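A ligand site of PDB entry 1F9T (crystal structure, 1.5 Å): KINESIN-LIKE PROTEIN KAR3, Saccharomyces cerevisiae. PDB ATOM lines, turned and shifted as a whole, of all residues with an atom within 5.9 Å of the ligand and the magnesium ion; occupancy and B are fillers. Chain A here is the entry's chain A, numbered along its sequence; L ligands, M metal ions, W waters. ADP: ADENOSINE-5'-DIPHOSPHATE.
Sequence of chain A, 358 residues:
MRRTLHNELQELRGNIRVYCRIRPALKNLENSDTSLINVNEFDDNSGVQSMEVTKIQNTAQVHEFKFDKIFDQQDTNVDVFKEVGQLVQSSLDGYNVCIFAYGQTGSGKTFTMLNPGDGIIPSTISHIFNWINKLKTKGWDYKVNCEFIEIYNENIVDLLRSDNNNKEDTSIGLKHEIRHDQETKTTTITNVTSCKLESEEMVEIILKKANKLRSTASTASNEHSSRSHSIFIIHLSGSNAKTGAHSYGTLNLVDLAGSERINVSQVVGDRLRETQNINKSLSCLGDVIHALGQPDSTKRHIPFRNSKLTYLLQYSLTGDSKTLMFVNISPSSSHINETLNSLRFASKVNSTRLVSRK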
ATOM      1  N   ARG A  21      17.243  20.272  14.812  1.00  0.00           N
ATOM      2  CA  ARG A  21      17.793  18.929  14.874  1.00  0.00           C
ATOM      3  C   ARG A  21      17.338  18.109  13.678  1.00  0.00           C
ATOM      4  O   ARG A  21      16.142  17.909  13.462  1.00  0.00           O
ATOM      5  CB  ARG A  21      17.372  18.205  16.144  1.00  0.00           C
ATOM      6  CG  ARG A  21      17.954  16.809  16.179  1.00  0.00           C
ATOM      7  CD  ARG A  21      17.310  15.892  17.194  1.00  0.00           C
ATOM      8  NE  ARG A  21      18.171  14.729  17.422  1.00  0.00           N
ATOM      9  CZ  ARG A  21      18.100  13.919  18.481  1.00  0.00           C
ATOM     10  NH1 ARG A  21      17.183  14.124  19.426  1.00  0.00           N
ATOM     11  NH2 ARG A  21      18.943  12.917  18.601  1.00  0.00           N
ATOM     12  N   ILE A  22      18.318  17.651  12.894  1.00  0.00           N
ATOM     13  CA  ILE A  22      18.043  16.812  11.738  1.00  0.00           C
ATOM     14  C   ILE A  22      18.188  15.381  12.219  1.00  0.00           C
ATOM     15  O   ILE A  22      19.254  14.974  12.665  1.00  0.00           O
ATOM     16  CB  ILE A  22      19.050  17.047  10.605  1.00  0.00           C
ATOM     17  CG1 ILE A  22      19.072  18.527  10.215  1.00  0.00           C
ATOM     18  CG2 ILE A  22      18.708  16.163   9.413  1.00  0.00           C
ATOM     19  CD1 ILE A  22      20.270  18.930   9.379  1.00  0.00           C
ATOM     20  N   ARG A  23      17.101  14.614  12.163  1.00  0.00           N
ATOM     21  CA  ARG A  23      17.178  13.237  12.615  1.00  0.00           C
ATOM     22  C   ARG A  23      17.801  12.394  11.518  1.00  0.00           C
ATOM     23  O   ARG A  23      17.832  12.801  10.354  1.00  0.00           O
ATOM     24  CB  ARG A  23      15.773  12.705  12.930  1.00  0.00           C
ATOM     25  CG  ARG A  23      14.872  12.546  11.721  1.00  0.00           C
ATOM     26  CD  ARG A  23      13.923  11.384  11.895  1.00  0.00           C
ATOM     27  NE  ARG A  23      12.781  11.474  10.991  1.00  0.00           N
ATOM     28  CZ  ARG A  23      12.810  11.056   9.734  1.00  0.00           C
ATOM     29  NH1 ARG A  23      13.910  10.507   9.249  1.00  0.00           N
ATOM     30  NH2 ARG A  23      11.733  11.181   8.960  1.00  0.00           N
ATOM     31  N   PRO A  24      18.336  11.221  11.882  1.00  0.00           N
ATOM     32  CA  PRO A  24      18.942  10.343  10.874  1.00  0.00           C
ATOM     33  C   PRO A  24      17.862   9.905   9.892  1.00  0.00           C
ATOM     34  O   PRO A  24      16.695   9.763  10.274  1.00  0.00           O
ATOM     35  CB  PRO A  24      19.467   9.166  11.688  1.00  0.00           C
ATOM     36  CG  PRO A  24      19.541   9.651  13.091  1.00  0.00           C
ATOM     37  CD  PRO A  24      18.437  10.654  13.239  1.00  0.00           C
ATOM     38  N   LEU A  26      15.488   7.589   7.618  1.00  0.00           N
ATOM     39  CA  LEU A  26      14.933   6.271   7.851  1.00  0.00           C
ATOM     40  C   LEU A  26      15.279   5.483   6.586  1.00  0.00           C
ATOM     41  O   LEU A  26      14.485   5.407   5.649  1.00  0.00           O
ATOM     42  CB  LEU A  26      13.414   6.349   8.048  1.00  0.00           C
ATOM     43  CG  LEU A  26      12.908   7.072   9.312  1.00  0.00           C
ATOM     44  CD1 LEU A  26      11.378   7.121   9.302  1.00  0.00           C
ATOM     45  CD2 LEU A  26      13.392   6.372  10.564  1.00  0.00           C
ATOM     46  N   ASP A  75      24.212  13.504  15.583  1.00  0.00           N
ATOM     47  CA  ASP A  75      23.984  13.875  16.976  1.00  0.00           C
ATOM     48  C   ASP A  75      22.920  12.984  17.623  1.00  0.00           C
ATOM     49  O   ASP A  75      21.768  12.965  17.194  1.00  0.00           O
ATOM     50  CB  ASP A  75      23.574  15.346  17.064  1.00  0.00           C
ATOM     51  CG  ASP A  75      24.750  16.274  16.867  1.00  0.00           C
ATOM     52  OD1 ASP A  75      25.773  16.084  17.550  1.00  0.00           O
ATOM     53  OD2 ASP A  75      24.643  17.189  16.021  1.00  0.00           O
ATOM     54  N   ASN A  77      20.804  11.528  21.160  1.00  0.00           N
ATOM     55  CA  ASN A  77      20.085  12.169  22.242  1.00  0.00           C
ATOM     56  C   ASN A  77      21.057  12.592  23.331  1.00  0.00           C
ATOM     57  O   ASN A  77      20.922  13.661  23.913  1.00  0.00           O
ATOM     58  CB  ASN A  77      19.024  11.214  22.787  1.00  0.00           C
ATOM     59  CG  ASN A  77      17.727  11.271  21.992  1.00  0.00           C
ATOM     60  OD1 ASN A  77      17.675  11.871  20.922  1.00  0.00           O
ATOM     61  ND2 ASN A  77      16.675  10.638  22.507  1.00  0.00           N
ATOM     62  N   GLY A 103       7.791  20.449  14.866  1.00  0.00           N
ATOM     63  CA  GLY A 103       8.110  19.789  13.602  1.00  0.00           C
ATOM     64  C   GLY A 103       6.971  18.940  13.064  1.00  0.00           C
ATOM     65  O   GLY A 103       6.003  18.669  13.779  1.00  0.00           O
ATOM     66  N   GLN A 104       7.077  18.517  11.821  1.00  0.00           N
ATOM     67  CA  GLN A 104       6.027  17.694  11.229  1.00  0.00           C
ATOM     68  C   GLN A 104       6.005  16.318  11.847  1.00  0.00           C
ATOM     69  O   GLN A 104       6.996  15.860  12.410  1.00  0.00           O
ATOM     70  CB  GLN A 104       6.229  17.566   9.718  1.00  0.00           C
ATOM     71  CG  GLN A 104       7.376  16.629   9.334  1.00  0.00           C
ATOM     72  CD  GLN A 104       7.542  16.498   7.829  1.00  0.00           C
ATOM     73  OE1 GLN A 104       6.595  16.127   7.117  1.00  0.00           O
ATOM     74  NE2 GLN A 104       8.736  16.797   7.338  1.00  0.00           N
ATOM     75  N   THR A 105       4.856  15.662  11.760  1.00  0.00           N
ATOM     76  CA  THR A 105       4.724  14.324  12.274  1.00  0.00           C
ATOM     77  C   THR A 105       5.784  13.503  11.549  1.00  0.00           C
ATOM     78  O   THR A 105       5.890  13.568  10.322  1.00  0.00           O
ATOM     79  CB  THR A 105       3.333  13.760  11.971  1.00  0.00           C
ATOM     80  OG1 THR A 105       2.345  14.559  12.638  1.00  0.00           O
ATOM     81  CG2 THR A 105       3.208  12.317  12.442  1.00  0.00           C
ATOM     82  N   GLY A 106       6.591  12.768  12.298  1.00  0.00           N
ATOM     83  CA  GLY A 106       7.626  11.959  11.693  1.00  0.00           C
ATOM     84  C   GLY A 106       9.025  12.558  11.778  1.00  0.00           C
ATOM     85  O   GLY A 106      10.006  11.872  11.475  1.00  0.00           O
ATOM     86  N   SER A 107       9.122  13.817  12.195  1.00  0.00           N
ATOM     87  CA  SER A 107      10.411  14.511  12.298  1.00  0.00           C
ATOM     88  C   SER A 107      11.278  14.127  13.511  1.00  0.00           C
ATOM     89  O   SER A 107      12.493  14.336  13.484  1.00  0.00           O
ATOM     90  CB  SER A 107      10.208  16.025  12.246  1.00  0.00           C
ATOM     91  OG  SER A 107       9.472  16.512  13.349  1.00  0.00           O
ATOM     92  N   GLY A 108      10.669  13.596  14.559  1.00  0.00           N
ATOM     93  CA  GLY A 108      11.433  13.192  15.732  1.00  0.00           C
ATOM     94  C   GLY A 108      11.147  13.916  17.046  1.00  0.00           C
ATOM     95  O   GLY A 108      11.951  13.839  17.977  1.00  0.00           O
ATOM     96  N   LYS A 109      10.004  14.589  17.139  1.00  0.00           N
ATOM     97  CA  LYS A 109       9.641  15.313  18.361  1.00  0.00           C
ATOM     98  C   LYS A 109       9.565  14.404  19.591  1.00  0.00           C
ATOM     99  O   LYS A 109      10.210  14.661  20.600  1.00  0.00           O
ATOM    100  CB  LYS A 109       8.306  16.033  18.187  1.00  0.00           C
ATOM    101  CG  LYS A 109       8.340  17.184  17.193  1.00  0.00           C
ATOM    102  CD  LYS A 109       6.970  17.839  17.022  1.00  0.00           C
ATOM    103  CE  LYS A 109       5.870  16.826  16.697  1.00  0.00           C
ATOM    104  NZ  LYS A 109       5.996  16.263  15.317  1.00  0.00           N
ATOM    105  N   THR A 110       8.788  13.330  19.487  1.00  0.00           N
ATOM    106  CA  THR A 110       8.649  12.416  20.608  1.00  0.00           C
ATOM    107  C   THR A 110       9.929  11.671  20.939  1.00  0.00           C
ATOM    108  O   THR A 110      10.260  11.486  22.109  1.00  0.00           O
ATOM    109  CB  THR A 110       7.524  11.416  20.348  1.00  0.00           C
ATOM    110  OG1 THR A 110       6.336  12.145  20.078  1.00  0.00           O
ATOM    111  CG2 THR A 110       7.289  10.519  21.564  1.00  0.00           C
ATOM    112  N   PHE A 111      10.643  11.242  19.908  1.00  0.00           N
ATOM    113  CA  PHE A 111      11.909  10.533  20.135  1.00  0.00           C
ATOM    114  C   PHE A 111      12.840  11.449  20.922  1.00  0.00           C
ATOM    115  O   PHE A 111      13.493  11.027  21.872  1.00  0.00           O
ATOM    116  CB  PHE A 111      12.567  10.176  18.805  1.00  0.00           C
ATOM    117  CG  PHE A 111      13.835   9.397  18.960  1.00  0.00           C
ATOM    118  CD1 PHE A 111      15.030  10.042  19.219  1.00  0.00           C
ATOM    119  CD2 PHE A 111      13.811   8.008  18.871  1.00  0.00           C
ATOM    120  CE1 PHE A 111      16.211   9.319  19.383  1.00  0.00           C
ATOM    121  CE2 PHE A 111      14.981   7.269  19.031  1.00  0.00           C
ATOM    122  CZ  PHE A 111      16.180   7.926  19.283  1.00  0.00           C
ATOM    123  N   THR A 112      12.894  12.715  20.518  1.00  0.00           N
ATOM    124  CA  THR A 112      13.729  13.708  21.158  1.00  0.00           C
ATOM    125  C   THR A 112      13.338  13.940  22.611  1.00  0.00           C
ATOM    126  O   THR A 112      14.203  14.030  23.494  1.00  0.00           O
ATOM    127  CB  THR A 112      13.631  15.050  20.401  1.00  0.00           C
ATOM    128  OG1 THR A 112      14.327  14.931  19.155  1.00  0.00           O
ATOM    129  CG2 THR A 112      14.259  16.187  21.222  1.00  0.00           C
ATOM    130  N   ARG A 214       2.473   8.260  23.878  1.00  0.00           N
ATOM    131  CA  ARG A 214       2.840   9.128  22.775  1.00  0.00           C
ATOM    132  C   ARG A 214       3.674   8.533  21.641  1.00  0.00           C
ATOM    133  O   ARG A 214       3.598   8.994  20.500  1.00  0.00           O
ATOM    134  CB  ARG A 214       3.542  10.364  23.333  1.00  0.00           C
ATOM    135  CG  ARG A 214       2.883  10.937  24.584  1.00  0.00           C
ATOM    136  CD  ARG A 214       1.414  11.234  24.339  1.00  0.00           C
ATOM    137  NE  ARG A 214       1.229  12.446  23.550  1.00  0.00           N
ATOM    138  CZ  ARG A 214       0.051  13.022  23.328  1.00  0.00           C
ATOM    139  NH1 ARG A 214      -1.065  12.485  23.829  1.00  0.00           N
ATOM    140  NH2 ARG A 214      -0.020  14.141  22.609  1.00  0.00           N
ATOM    141  N   SER A 215       4.476   7.524  21.954  1.00  0.00           N
ATOM    142  CA  SER A 215       5.304   6.892  20.938  1.00  0.00           C
ATOM    143  C   SER A 215       4.427   6.148  19.944  1.00  0.00           C
ATOM    144  O   SER A 215       3.232   5.961  20.183  1.00  0.00           O
ATOM    145  CB  SER A 215       6.292   5.915  21.573  1.00  0.00           C
ATOM    146  OG  SER A 215       7.614   6.215  21.174  1.00  0.00           O
ATOM    147  N   THR A 216       5.007   5.719  18.833  1.00  0.00           N
ATOM    148  CA  THR A 216       4.242   5.015  17.818  1.00  0.00           C
ATOM    149  C   THR A 216       4.332   3.504  17.973  1.00  0.00           C
ATOM    150  O   THR A 216       5.345   2.886  17.656  1.00  0.00           O
ATOM    151  CB  THR A 216       4.683   5.393  16.396  1.00  0.00           C
ATOM    152  OG1 THR A 216       5.493   6.569  16.445  1.00  0.00           O
ATOM    153  CG2 THR A 216       3.461   5.672  15.540  1.00  0.00           C
ATOM    154  N   SER A 225      -2.154  11.522  19.186  1.00  0.00           N
ATOM    155  CA  SER A 225      -0.930  12.132  19.665  1.00  0.00           C
ATOM    156  C   SER A 225      -0.349  13.134  18.677  1.00  0.00           C
ATOM    157  O   SER A 225       0.184  14.172  19.052  1.00  0.00           O
ATOM    158  CB  SER A 225       0.110  11.044  19.948  1.00  0.00           C
ATOM    159  OG  SER A 225      -0.402  10.051  20.804  1.00  0.00           O
ATOM    160  N   SER A 226      -0.462  12.821  17.383  1.00  0.00           N
ATOM    161  CA  SER A 226       0.067  13.696  16.356  1.00  0.00           C
ATOM    162  C   SER A 226      -0.739  14.980  16.240  1.00  0.00           C
ATOM    163  O   SER A 226      -0.239  15.983  15.731  1.00  0.00           O
ATOM    164  CB  SER A 226       0.068  12.975  15.009  1.00  0.00           C
ATOM    165  OG  SER A 226      -1.242  12.936  14.443  1.00  0.00           O
ATOM    166  N   ASP A 255       5.819  18.501  23.763  1.00  0.00           N
ATOM    167  CA  ASP A 255       5.885  17.723  22.522  1.00  0.00           C
ATOM    168  C   ASP A 255       4.658  18.229  21.756  1.00  0.00           C
ATOM    169  O   ASP A 255       3.529  17.789  21.991  1.00  0.00           O
ATOM    170  CB  ASP A 255       5.756  16.239  22.868  1.00  0.00           C
ATOM    171  CG  ASP A 255       5.814  15.337  21.656  1.00  0.00           C
ATOM    172  OD1 ASP A 255       5.963  15.841  20.525  1.00  0.00           O
ATOM    173  OD2 ASP A 255       5.717  14.104  21.842  1.00  0.00           O
ATOM    174  N   ASN A 328      12.480  20.149  14.956  1.00  0.00           N
ATOM    175  CA  ASN A 328      12.826  18.845  14.400  1.00  0.00           C
ATOM    176  C   ASN A 328      12.488  18.793  12.908  1.00  0.00           C
ATOM    177  O   ASN A 328      11.409  19.211  12.502  1.00  0.00           O
ATOM    178  CB  ASN A 328      12.064  17.733  15.122  1.00  0.00           C
ATOM    179  CG  ASN A 328      12.434  17.623  16.587  1.00  0.00           C
ATOM    180  OD1 ASN A 328      11.765  18.195  17.456  1.00  0.00           O
ATOM    181  ND2 ASN A 328      13.500  16.886  16.871  1.00  0.00           N
HETATM  182  PB  ADP L   1       7.272  12.744  15.647  1.00  0.00           P
HETATM  183  O1B ADP L   1       7.813  14.054  15.227  1.00  0.00           O
HETATM  184  O2B ADP L   1       7.112  12.672  17.257  1.00  0.00           O
HETATM  185  O3B ADP L   1       5.998  12.435  14.923  1.00  0.00           O
HETATM  186  PA  ADP L   1       8.770  10.336  16.198  1.00  0.00           P
HETATM  187  O1A ADP L   1       9.629  10.781  17.310  1.00  0.00           O
HETATM  188  O2A ADP L   1       7.636   9.572  16.724  1.00  0.00           O
HETATM  189  O3A ADP L   1       8.303  11.591  15.358  1.00  0.00           O
HETATM  190  O5' ADP L   1       9.561   9.361  15.232  1.00  0.00           O
HETATM  191  C5' ADP L   1       9.796   9.468  13.827  1.00  0.00           C
HETATM  192  C4' ADP L   1      10.543   8.146  13.503  1.00  0.00           C
HETATM  193  O4' ADP L   1      11.918   8.506  13.423  1.00  0.00           O
HETATM  194  C3' ADP L   1      10.468   7.108  14.649  1.00  0.00           C
HETATM  195  O3' ADP L   1      10.390   5.750  14.178  1.00  0.00           O
HETATM  196  C2' ADP L   1      11.731   7.338  15.476  1.00  0.00           C
HETATM  197  O2' ADP L   1      12.159   6.184  16.211  1.00  0.00           O
HETATM  198  C1' ADP L   1      12.709   7.875  14.446  1.00  0.00           C
HETATM  199  N9  ADP L   1      13.606   8.930  15.009  1.00  0.00           N
HETATM  200  C8  ADP L   1      13.224  10.188  15.293  1.00  0.00           C
HETATM  201  N7  ADP L   1      14.266  10.863  15.751  1.00  0.00           N
HETATM  202  C5  ADP L   1      15.312  10.073  15.755  1.00  0.00           C
HETATM  203  C6  ADP L   1      16.647  10.205  16.121  1.00  0.00           C
HETATM  204  N6  ADP L   1      17.110  11.372  16.563  1.00  0.00           N
HETATM  205  N1  ADP L   1      17.486   9.130  15.993  1.00  0.00           N
HETATM  206  C2  ADP L   1      17.066   7.936  15.543  1.00  0.00           C
HETATM  207  N3  ADP L   1      15.772   7.795  15.197  1.00  0.00           N
HETATM  208  C4  ADP L   1      14.883   8.816  15.281  1.00  0.00           C
HETATM  209 MG    MG M   1       5.146  12.166  18.269  1.00  0.00          MG
HETATM  210  O   HOH W   1       4.739  14.343  18.633  1.00  0.00           O
HETATM  211  O   HOH W   2      15.160  13.443  16.475  1.00  0.00           O
HETATM  212  O   HOH W   3       8.653   8.551  19.135  1.00  0.00           O
HETATM  213  O   HOH W   4       5.607   9.964  18.059  1.00  0.00           O
HETATM  214  O   HOH W   5      20.086   8.985  17.086  1.00  0.00           O
HETATM  215  O   HOH W   6       5.401   9.788  14.261  1.00  0.00           O
HETATM  216  O   HOH W   7       3.326  11.533  19.494  1.00  0.00           O
HETATM  217  O   HOH W   8       3.742  12.310  16.490  1.00  0.00           O
HETATM  218  O   HOH W   9      14.831   4.699  15.324  1.00  0.00           O
HETATM  219  O   HOH W  10      10.588   5.976  18.502  1.00  0.00           O
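One residue has an atom within 4 Å of the magnesium ion: Thr 110. The nearest printed residue that does not touch the magnesium ion is Asp 255 (4.1 Å).
The side-chain hydroxyl (OG1) of Thr 110 lies close to the side-chain carboxylate (OD2) of Asp 255 (2.7 Å). The backbone carbonyl oxygen (O) of Gly 106 sits at hydrogen-bond distance from the guanidinium group (NE) of Arg 23 (2.8 Å). The backbone carbonyl oxygen (O) of Gly 103 sits at hydrogen-bond distance from the side-chain amino group (NZ) of Lys 109. O of Gly 108 sits at hydrogen-bond distance from OG1 of Thr 112 (2.9 Å). The guanidinium group of Arg 21 sits at hydrogen-bond distance from the side-chain amide oxygen of Asn 77, at 2.7 Å. O of Asp 75 lies within hydrogen-bond range of NH2 of Arg 21. The guanidinium group (NH1) of Arg 21 lies within hydrogen-bond range of the side-chain hydroxyl (OG1) of Thr 112, at 3.0 Å. The side-chain hydroxyl of Ser 107 lies close to the backbone carbonyl oxygen of Asn 328 (3.4 Å).
The backbone NH of Thr 110 lies within hydrogen-bond range of an oxygen (O1A) of the ligand (3.5 Å). An oxygen (O3B) of the ligand sits at hydrogen-bond distance from the backbone NH (N) of Gly 106 (2.7 Å). The backbone NH of Phe 111 sits at hydrogen-bond distance from an oxygen (O1A) of the ligand (2.8 Å). The backbone NH (N) of Lys 109 is in hydrogen-bond range of an oxygen (O1B) of the ligand (3.0 Å). An oxygen (O1B) of the ligand lies within salt-bridge range of the side-chain amino group (NZ) of Lys 109 (2.9 Å). N of Gly 108 lies within hydrogen-bond range of O1B of the ligand (3.0 Å). N of Ser 107 is in hydrogen-bond range of O1B of the ligand (3.3 Å).
A nitrogen (N6) of the ligand lies close to the guanidinium group (NH2) of Arg 21, at 3.1 Å. O of Gln 104 lies close to O1B of the ligand (3.4 Å). Arg 23 touches the ligand (CD to C8, 3.7 Å). Pro 24 touches the ligand. Leu 26 touches the ligand. CA of Thr 105 touches O3B of the ligand, at 3.5 Å. Thr 216 touches the ligand (OG1 to O2A, 3.7 Å).
The magnesium ion is bound by the side-chain hydroxyl of Thr 110 (2.2 Å), water W1 (2.2 Å), water W4 (2.3 Å), an oxygen (O2B) of the ligand (2.3 Å), water W8 (2.3 Å) and water W7 (2.3 Å).
Water W4 bridges an oxygen (O2A) of the ligand (2.5 Å) and the backbone carbonyl oxygen of Arg 214 (3.3 Å). Water W3 lies within hydrogen-bond range of O2A of the ligand (2.8 Å), OG of Ser 215 (3.3 Å) and N of Phe 111 (3.4 Å). Water W2 lies within hydrogen-bond range of N7 of the ligand, OG1 of Thr 112 and NE of Arg 21.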
